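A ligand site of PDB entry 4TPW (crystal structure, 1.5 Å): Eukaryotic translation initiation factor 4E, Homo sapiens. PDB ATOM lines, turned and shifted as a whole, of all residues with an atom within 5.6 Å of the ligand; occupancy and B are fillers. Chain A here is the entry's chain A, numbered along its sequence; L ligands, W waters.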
ATOM      1  N   PHE A  22      -2.421  12.480  -2.172  1.00  0.00           N
ATOM      2  CA  PHE A  22      -2.171  12.511  -3.615  1.00  0.00           C
ATOM      3  C   PHE A  22      -2.519  13.879  -4.181  1.00  0.00           C
ATOM      4  O   PHE A  22      -3.599  14.399  -3.908  1.00  0.00           O
ATOM      5  CB  PHE A  22      -2.974  11.421  -4.314  1.00  0.00           C
ATOM      6  CG  PHE A  22      -2.787  11.385  -5.802  1.00  0.00           C
ATOM      7  CD1 PHE A  22      -1.847  10.537  -6.372  1.00  0.00           C
ATOM      8  CD2 PHE A  22      -3.538  12.190  -6.643  1.00  0.00           C
ATOM      9  CE1 PHE A  22      -1.667  10.493  -7.739  1.00  0.00           C
ATOM     10  CE2 PHE A  22      -3.364  12.151  -8.004  1.00  0.00           C
ATOM     11  CZ  PHE A  22      -2.422  11.306  -8.557  1.00  0.00           C
ATOM     12  N   ASN A  24      -3.027  15.851  -7.711  1.00  0.00           N
ATOM     13  CA  ASN A  24      -3.214  15.707  -9.151  1.00  0.00           C
ATOM     14  C   ASN A  24      -2.230  16.525  -9.962  1.00  0.00           C
ATOM     15  O   ASN A  24      -1.999  17.703  -9.692  1.00  0.00           O
ATOM     16  CB  ASN A  24      -4.640  16.102  -9.544  1.00  0.00           C
ATOM     17  CG  ASN A  24      -5.626  14.971  -9.356  1.00  0.00           C
ATOM     18  OD1 ASN A  24      -6.164  14.438 -10.323  1.00  0.00           O
ATOM     19  ND2 ASN A  24      -5.853  14.579  -8.106  1.00  0.00           N
ATOM     20  N   TRP A  30       1.708   9.339 -12.802  1.00  0.00           N
ATOM     21  CA  TRP A  30       0.754   9.245 -11.697  1.00  0.00           C
ATOM     22  C   TRP A  30       1.392   8.877 -10.364  1.00  0.00           C
ATOM     23  O   TRP A  30       1.097   9.502  -9.339  1.00  0.00           O
ATOM     24  CB  TRP A  30      -0.340   8.217 -12.045  1.00  0.00           C
ATOM     25  CG  TRP A  30      -1.474   8.185 -11.070  1.00  0.00           C
ATOM     26  CD1 TRP A  30      -2.603   8.950 -11.100  1.00  0.00           C
ATOM     27  CD2 TRP A  30      -1.597   7.332  -9.923  1.00  0.00           C
ATOM     28  NE1 TRP A  30      -3.423   8.642 -10.039  1.00  0.00           N
ATOM     29  CE2 TRP A  30      -2.821   7.647  -9.300  1.00  0.00           C
ATOM     30  CE3 TRP A  30      -0.790   6.343  -9.358  1.00  0.00           C
ATOM     31  CZ2 TRP A  30      -3.263   7.003  -8.149  1.00  0.00           C
ATOM     32  CZ3 TRP A  30      -1.232   5.705  -8.215  1.00  0.00           C
ATOM     33  CH2 TRP A  30      -2.452   6.036  -7.618  1.00  0.00           C
ATOM     34  N   GLN A  31       2.249   7.865 -10.380  1.00  0.00           N
ATOM     35  CA  GLN A  31       2.885   7.352  -9.164  1.00  0.00           C
ATOM     36  C   GLN A  31       3.698   8.426  -8.440  1.00  0.00           C
ATOM     37  O   GLN A  31       3.862   8.385  -7.224  1.00  0.00           O
ATOM     38  CB  GLN A  31       3.788   6.161  -9.491  1.00  0.00           C
ATOM     39  CG  GLN A  31       3.079   4.935 -10.053  1.00  0.00           C
ATOM     40  CD  GLN A  31       2.888   5.012 -11.555  1.00  0.00           C
ATOM     41  OE1 GLN A  31       2.455   6.037 -12.085  1.00  0.00           O
ATOM     42  NE2 GLN A  31       3.197   3.928 -12.246  1.00  0.00           N
ATOM     43  N   ASP A  64      -6.224  14.139  -3.161  1.00  0.00           N
ATOM     44  CA  ASP A  64      -6.908  12.954  -2.664  1.00  0.00           C
ATOM     45  C   ASP A  64      -6.275  12.378  -1.412  1.00  0.00           C
ATOM     46  O   ASP A  64      -5.064  12.522  -1.193  1.00  0.00           O
ATOM     47  CB  ASP A  64      -6.954  11.883  -3.756  1.00  0.00           C
ATOM     48  CG  ASP A  64      -7.508  12.418  -5.058  1.00  0.00           C
ATOM     49  OD1 ASP A  64      -7.996  13.564  -5.064  1.00  0.00           O
ATOM     50  OD2 ASP A  64      -7.462  11.682  -6.067  1.00  0.00           O
ATOM     51  N   PRO A  74      -1.735   2.460  -2.383  1.00  0.00           N
ATOM     52  CA  PRO A  74      -3.066   2.782  -2.917  1.00  0.00           C
ATOM     53  C   PRO A  74      -3.051   2.989  -4.427  1.00  0.00           C
ATOM     54  O   PRO A  74      -3.452   4.027  -4.933  1.00  0.00           O
ATOM     55  CB  PRO A  74      -3.411   4.081  -2.177  1.00  0.00           C
ATOM     56  CG  PRO A  74      -2.104   4.741  -1.979  1.00  0.00           C
ATOM     57  CD  PRO A  74      -1.122   3.632  -1.722  1.00  0.00           C
ATOM     58  N   MET A  75      -2.593   1.957  -5.140  1.00  0.00           N
ATOM     59  CA  MET A  75      -2.508   2.005  -6.589  1.00  0.00           C
ATOM     60  C   MET A  75      -2.816   0.632  -7.187  1.00  0.00           C
ATOM     61  O   MET A  75      -2.582  -0.390  -6.533  1.00  0.00           O
ATOM     62  CB  MET A  75      -1.117   2.485  -7.019  1.00  0.00           C
ATOM     63  CG  MET A  75       0.040   1.619  -6.526  1.00  0.00           C
ATOM     64  SD  MET A  75       1.667   2.317  -6.907  1.00  0.00           S
ATOM     65  CE  MET A  75       1.700   3.743  -5.829  1.00  0.00           C
ATOM     66  N   TRP A  76      -3.345   0.614  -8.406  1.00  0.00           N
ATOM     67  CA  TRP A  76      -3.679  -0.629  -9.112  1.00  0.00           C
ATOM     68  C   TRP A  76      -2.518  -1.612  -9.148  1.00  0.00           C
ATOM     69  O   TRP A  76      -2.718  -2.831  -9.108  1.00  0.00           O
ATOM     70  CB  TRP A  76      -4.090  -0.337 -10.560  1.00  0.00           C
ATOM     71  CG  TRP A  76      -5.214   0.605 -10.740  1.00  0.00           C
ATOM     72  CD1 TRP A  76      -6.301   0.783  -9.915  1.00  0.00           C
ATOM     73  CD2 TRP A  76      -5.390   1.509 -11.830  1.00  0.00           C
ATOM     74  NE1 TRP A  76      -7.131   1.748 -10.431  1.00  0.00           N
ATOM     75  CE2 TRP A  76      -6.595   2.206 -11.607  1.00  0.00           C
ATOM     76  CE3 TRP A  76      -4.645   1.805 -12.980  1.00  0.00           C
ATOM     77  CZ2 TRP A  76      -7.065   3.180 -12.495  1.00  0.00           C
ATOM     78  CZ3 TRP A  76      -5.114   2.765 -13.854  1.00  0.00           C
ATOM     79  CH2 TRP A  76      -6.309   3.445 -13.606  1.00  0.00           C
ATOM     80  N   GLU A  77      -1.300  -1.070  -9.255  1.00  0.00           N
ATOM     81  CA  GLU A  77      -0.089  -1.864  -9.419  1.00  0.00           C
ATOM     82  C   GLU A  77       0.167  -2.851  -8.307  1.00  0.00           C
ATOM     83  O   GLU A  77       0.799  -3.894  -8.526  1.00  0.00           O
ATOM     84  CB  GLU A  77       1.126  -0.935  -9.523  1.00  0.00           C
ATOM     85  CG  GLU A  77       1.092  -0.067 -10.736  1.00  0.00           C
ATOM     86  CD  GLU A  77       0.503   1.302 -10.480  1.00  0.00           C
ATOM     87  OE1 GLU A  77      -0.697   1.368 -10.165  1.00  0.00           O
ATOM     88  OE2 GLU A  77       1.246   2.295 -10.608  1.00  0.00           O
ATOM     89  N   ARG A  86     -13.118  -1.742  -7.154  1.00  0.00           N
ATOM     90  CA  ARG A  86     -13.637  -0.785  -6.184  1.00  0.00           C
ATOM     91  C   ARG A  86     -15.136  -0.576  -6.287  1.00  0.00           C
ATOM     92  O   ARG A  86     -15.700  -0.577  -7.386  1.00  0.00           O
ATOM     93  CB  ARG A  86     -12.931   0.554  -6.345  1.00  0.00           C
ATOM     94  CG  ARG A  86     -13.203   1.204  -7.678  1.00  0.00           C
ATOM     95  CD  ARG A  86     -12.544   2.566  -7.825  1.00  0.00           C
ATOM     96  NE  ARG A  86     -12.756   3.076  -9.177  1.00  0.00           N
ATOM     97  CZ  ARG A  86     -12.563   4.328  -9.565  1.00  0.00           C
ATOM     98  NH1 ARG A  86     -12.126   5.237  -8.694  1.00  0.00           N
ATOM     99  NH2 ARG A  86     -12.794   4.671 -10.826  1.00  0.00           N
ATOM    100  N   ASN A 129     -11.556  11.155  -3.748  1.00  0.00           N
ATOM    101  CA  ASN A 129     -11.103  12.083  -4.773  1.00  0.00           C
ATOM    102  C   ASN A 129     -11.890  13.377  -4.668  1.00  0.00           C
ATOM    103  O   ASN A 129     -13.119  13.376  -4.756  1.00  0.00           O
ATOM    104  CB  ASN A 129     -11.275  11.506  -6.179  1.00  0.00           C
ATOM    105  CG  ASN A 129     -10.730  10.090  -6.321  1.00  0.00           C
ATOM    106  OD1 ASN A 129     -11.487   9.150  -6.550  1.00  0.00           O
ATOM    107  ND2 ASN A 129      -9.420   9.936  -6.198  1.00  0.00           N
ATOM    108  N   ARG A 131     -12.833  16.539  -6.564  1.00  0.00           N
ATOM    109  CA  ARG A 131     -12.877  16.996  -7.945  1.00  0.00           C
ATOM    110  C   ARG A 131     -13.982  18.029  -8.150  1.00  0.00           C
ATOM    111  O   ARG A 131     -15.089  17.867  -7.634  1.00  0.00           O
ATOM    112  CB  ARG A 131     -13.121  15.814  -8.899  1.00  0.00           C
ATOM    113  CG  ARG A 131     -12.116  14.686  -8.806  1.00  0.00           C
ATOM    114  CD  ARG A 131     -10.818  15.015  -9.518  1.00  0.00           C
ATOM    115  NE  ARG A 131      -9.903  13.874  -9.512  1.00  0.00           N
ATOM    116  CZ  ARG A 131      -9.070  13.579  -8.513  1.00  0.00           C
ATOM    117  NH1 ARG A 131      -9.022  14.354  -7.433  1.00  0.00           N
ATOM    118  NH2 ARG A 131      -8.286  12.516  -8.599  1.00  0.00           N
ATOM    119  N   LYS A 133     -15.439  18.387 -10.802  1.00  0.00           N
ATOM    120  CA  LYS A 133     -16.393  17.617 -11.604  1.00  0.00           C
ATOM    121  C   LYS A 133     -17.410  16.911 -10.719  1.00  0.00           C
ATOM    122  O   LYS A 133     -18.540  16.646 -11.139  1.00  0.00           O
ATOM    123  CB  LYS A 133     -15.640  16.612 -12.465  1.00  0.00           C
ATOM    124  CG  LYS A 133     -16.449  15.985 -13.594  1.00  0.00           C
ATOM    125  CD  LYS A 133     -15.567  15.089 -14.460  1.00  0.00           C
ATOM    126  CE  LYS A 133     -14.539  15.885 -15.256  1.00  0.00           C
ATOM    127  NZ  LYS A 133     -13.583  15.005 -15.988  1.00  0.00           N
ATOM    128  N   LYS A 136     -15.563  11.907  -5.335  1.00  0.00           N
ATOM    129  CA  LYS A 136     -15.761  10.467  -5.374  1.00  0.00           C
ATOM    130  C   LYS A 136     -15.179   9.811  -4.126  1.00  0.00           C
ATOM    131  O   LYS A 136     -14.149  10.233  -3.609  1.00  0.00           O
ATOM    132  CB  LYS A 136     -15.116   9.869  -6.625  1.00  0.00           C
ATOM    133  CG  LYS A 136     -15.755  10.347  -7.918  1.00  0.00           C
ATOM    134  CD  LYS A 136     -15.085   9.743  -9.135  1.00  0.00           C
ATOM    135  CE  LYS A 136     -13.695  10.310  -9.351  1.00  0.00           C
ATOM    136  NZ  LYS A 136     -13.101   9.804 -10.617  1.00  0.00           N
ATOM    137  N   TRP A 140     -11.770  -0.069  -2.025  1.00  0.00           N
ATOM    138  CA  TRP A 140     -11.013  -0.978  -2.862  1.00  0.00           C
ATOM    139  C   TRP A 140     -10.949  -2.360  -2.235  1.00  0.00           C
ATOM    140  O   TRP A 140     -10.654  -2.483  -1.045  1.00  0.00           O
ATOM    141  CB  TRP A 140      -9.595  -0.453  -3.080  1.00  0.00           C
ATOM    142  CG  TRP A 140      -9.465   0.743  -3.970  1.00  0.00           C
ATOM    143  CD1 TRP A 140     -10.367   1.742  -4.147  1.00  0.00           C
ATOM    144  CD2 TRP A 140      -8.348   1.042  -4.819  1.00  0.00           C
ATOM    145  NE1 TRP A 140      -9.879   2.662  -5.056  1.00  0.00           N
ATOM    146  CE2 TRP A 140      -8.638   2.254  -5.476  1.00  0.00           C
ATOM    147  CE3 TRP A 140      -7.126   0.410  -5.078  1.00  0.00           C
ATOM    148  CZ2 TRP A 140      -7.768   2.846  -6.387  1.00  0.00           C
ATOM    149  CZ3 TRP A 140      -6.261   1.000  -5.976  1.00  0.00           C
ATOM    150  CH2 TRP A 140      -6.579   2.205  -6.623  1.00  0.00           C
ATOM    151  N   LYS A 180      -9.768   2.167 -19.534  1.00  0.00           N
ATOM    152  CA  LYS A 180     -10.780   3.155 -19.907  1.00  0.00           C
ATOM    153  C   LYS A 180     -10.787   4.318 -18.902  1.00  0.00           C
ATOM    154  O   LYS A 180      -9.771   5.000 -18.748  1.00  0.00           O
ATOM    155  CB  LYS A 180     -12.166   2.492 -20.000  1.00  0.00           C
ATOM    156  CG  LYS A 180     -12.402   1.678 -21.268  1.00  0.00           C
ATOM    157  CD  LYS A 180     -12.303   2.501 -22.555  1.00  0.00           C
ATOM    158  CE  LYS A 180     -13.376   3.592 -22.620  1.00  0.00           C
ATOM    159  NZ  LYS A 180     -13.201   4.462 -23.813  1.00  0.00           N
ATOM    160  N   SER A 181     -11.912   4.557 -18.224  1.00  0.00           N
ATOM    161  CA  SER A 181     -12.028   5.665 -17.290  1.00  0.00           C
ATOM    162  C   SER A 181     -13.123   5.372 -16.268  1.00  0.00           C
ATOM    163  O   SER A 181     -14.117   4.736 -16.592  1.00  0.00           O
ATOM    164  CB  SER A 181     -12.342   6.969 -18.037  1.00  0.00           C
ATOM    165  OG  SER A 181     -13.696   7.001 -18.447  1.00  0.00           O
ATOM    166  N   GLY A 182     -12.923   5.824 -15.032  1.00  0.00           N
ATOM    167  CA  GLY A 182     -13.826   5.503 -13.946  1.00  0.00           C
ATOM    168  C   GLY A 182     -15.271   5.869 -14.197  1.00  0.00           C
ATOM    169  O   GLY A 182     -16.167   5.362 -13.510  1.00  0.00           O
ATOM    170  N   SER A 183     -15.510   6.757 -15.169  1.00  0.00           N
ATOM    171  CA  SER A 183     -16.868   7.155 -15.525  1.00  0.00           C
ATOM    172  C   SER A 183     -17.446   6.256 -16.611  1.00  0.00           C
ATOM    173  O   SER A 183     -18.585   5.800 -16.511  1.00  0.00           O
ATOM    174  CB  SER A 183     -16.894   8.634 -15.973  1.00  0.00           C
ATOM    175  OG  SER A 183     -15.960   8.855 -17.021  1.00  0.00           O
HETATM  176  P1  LIG L   1      -8.746   9.267 -11.079  1.00  0.00           P
HETATM  177  O1  LIG L   1      -8.041  10.400 -10.370  1.00  0.00           O
HETATM  178  O2  LIG L   1      -8.947   8.110 -10.128  1.00  0.00           O
HETATM  179  O3  LIG L   1     -10.169   9.740 -11.623  1.00  0.00           O
HETATM  180  O4  LIG L   1      -7.865   8.740 -12.271  1.00  0.00           O
HETATM  181  P2  LIG L   1     -10.504  11.166 -12.259  1.00  0.00           P
HETATM  182  O5  LIG L   1      -9.368  12.116 -12.021  1.00  0.00           O
HETATM  183  O6  LIG L   1     -11.761  11.709 -11.631  1.00  0.00           O
HETATM  184  O7  LIG L   1     -10.728  11.010 -13.834  1.00  0.00           O
HETATM  185  P3  LIG L   1     -11.458   9.795 -14.567  1.00  0.00           P
HETATM  186  O8  LIG L   1     -11.578   8.600 -13.649  1.00  0.00           O
HETATM  187  O9  LIG L   1     -10.657   9.408 -15.780  1.00  0.00           O
HETATM  188  O10 LIG L   1     -12.847  10.225 -15.001  1.00  0.00           O
HETATM  189  C1  LIG L   1      -7.483   9.613 -13.343  1.00  0.00           C
HETATM  190  C2  LIG L   1      -6.404   8.908 -14.126  1.00  0.00           C
HETATM  191  O11 LIG L   1      -5.103   8.621 -13.086  1.00  0.00           O
HETATM  192  C3  LIG L   1      -6.771   7.791 -14.532  1.00  0.00           C
HETATM  193  O12 LIG L   1      -7.409   7.883 -15.898  1.00  0.00           O
HETATM  194  C4  LIG L   1      -5.430   6.975 -14.620  1.00  0.00           C
HETATM  195  O13 LIG L   1      -4.810   7.258 -15.740  1.00  0.00           O
HETATM  196  C5  LIG L   1      -4.577   7.488 -13.412  1.00  0.00           C
HETATM  197  N1  LIG L   1      -4.715   6.580 -12.318  1.00  0.00           N
HETATM  198  C6  LIG L   1      -5.694   6.525 -11.411  1.00  0.00           C
HETATM  199  N2  LIG L   1      -5.447   5.549 -10.542  1.00  0.00           N
HETATM  200  C7  LIG L   1      -6.281   5.173  -9.420  1.00  0.00           C
HETATM  201  C8  LIG L   1      -4.270   4.938 -10.889  1.00  0.00           C
HETATM  202  C9  LIG L   1      -3.457   3.803 -10.328  1.00  0.00           C
HETATM  203  O14 LIG L   1      -3.840   3.201  -9.340  1.00  0.00           O
HETATM  204  N3  LIG L   1      -2.270   3.425 -10.953  1.00  0.00           N
HETATM  205  C10 LIG L   1      -1.793   4.122 -12.111  1.00  0.00           C
HETATM  206  N4  LIG L   1      -0.570   3.731 -12.738  1.00  0.00           N
HETATM  207  N5  LIG L   1      -2.576   5.219 -12.657  1.00  0.00           N
HETATM  208  C11 LIG L   1      -3.812   5.602 -12.021  1.00  0.00           C
HETATM  209  O   HOH W   1      -8.924   5.031 -16.107  1.00  0.00           O
HETATM  210  O   HOH W   2     -10.538   6.369 -14.051  1.00  0.00           O
HETATM  211  O   HOH W   3      -2.062   5.731 -15.577  1.00  0.00           O
HETATM  212  O   HOH W   4     -11.446   7.972  -9.005  1.00  0.00           O
HETATM  213  O   HOH W   5      -9.338   5.725 -11.428  1.00  0.00           O
HETATM  214  O   HOH W   6      -8.999   6.623  -7.482  1.00  0.00           O
HETATM  215  O   HOH W   7     -13.457  13.558 -12.131  1.00  0.00           O
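Gln 31 touches the ligand. CA of Met 75 touches O14 of the ligand, at 3.3 Å. Trp 140 touches the ligand. CB of Ser 181 touches O9 of the ligand, at 3.7 Å. OG of Ser 183 touches O10 of the ligand, at 3.96 Å. Hydrophobic or aromatic side chains that line the ligand: Trp 30, Met 75, Trp 76 and Trp 140. Of the 19 residues printed, 11 come within 4 Å of the ligand. The nearest printed residue that does not touch the ligand is Asn 24 (4.3 Å).
Water W2 lies within hydrogen-bond range of O8 of the ligand and N of Gly 182. Water W4 lies within hydrogen-bond range of the side-chain amide oxygen of Asn 129 (2.7 Å), an oxygen (O2) of the ligand (2.7 Å), the guanidinium group of Arg 86 (2.8 Å) and the side-chain amino group of Lys 136 (2.9 Å). Water W1 lies within hydrogen-bond range of O of Lys 180 (2.8 Å) and O12 of the ligand (3.2 Å).
NH1 of Arg 131 lies within salt-bridge range of OD1 of Asp 64 (2.7 Å). OG of Ser 181 is in hydrogen-bond range of OG of Ser 183 (3.3 Å). The side-chain amide nitrogen of Asn 24 lies close to the guanidinium group of Arg 131, 3.2 Å away. OE2 of Glu 77 sits at hydrogen-bond distance from NE2 of Gln 31, at 3.0 Å. The backbone NH (N) of Asn 129 is in hydrogen-bond range of the backbone carbonyl oxygen (O) of Lys 136 (2.8 Å).
The side-chain amino group (NZ) of Lys 136 is in salt-bridge range of an oxygen (O6) of the ligand (2.5 Å). The guanidinium group (NH2) of Arg 131 lies within salt-bridge range of an oxygen (O1) of the ligand, at 2.8 Å. An oxygen (O8) of the ligand sits at hydrogen-bond distance from the backbone NH of Gly 182 (3.4 Å). A nitrogen (N3) of the ligand lies within hydrogen-bond range of the side-chain carboxylate of Glu 77, at 2.7 Å. An oxygen (O14) of the ligand is in hydrogen-bond range of the backbone NH of Trp 76 (2.8 Å). O11 of the ligand lies close to NE1 of Trp 30 (3.5 Å).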
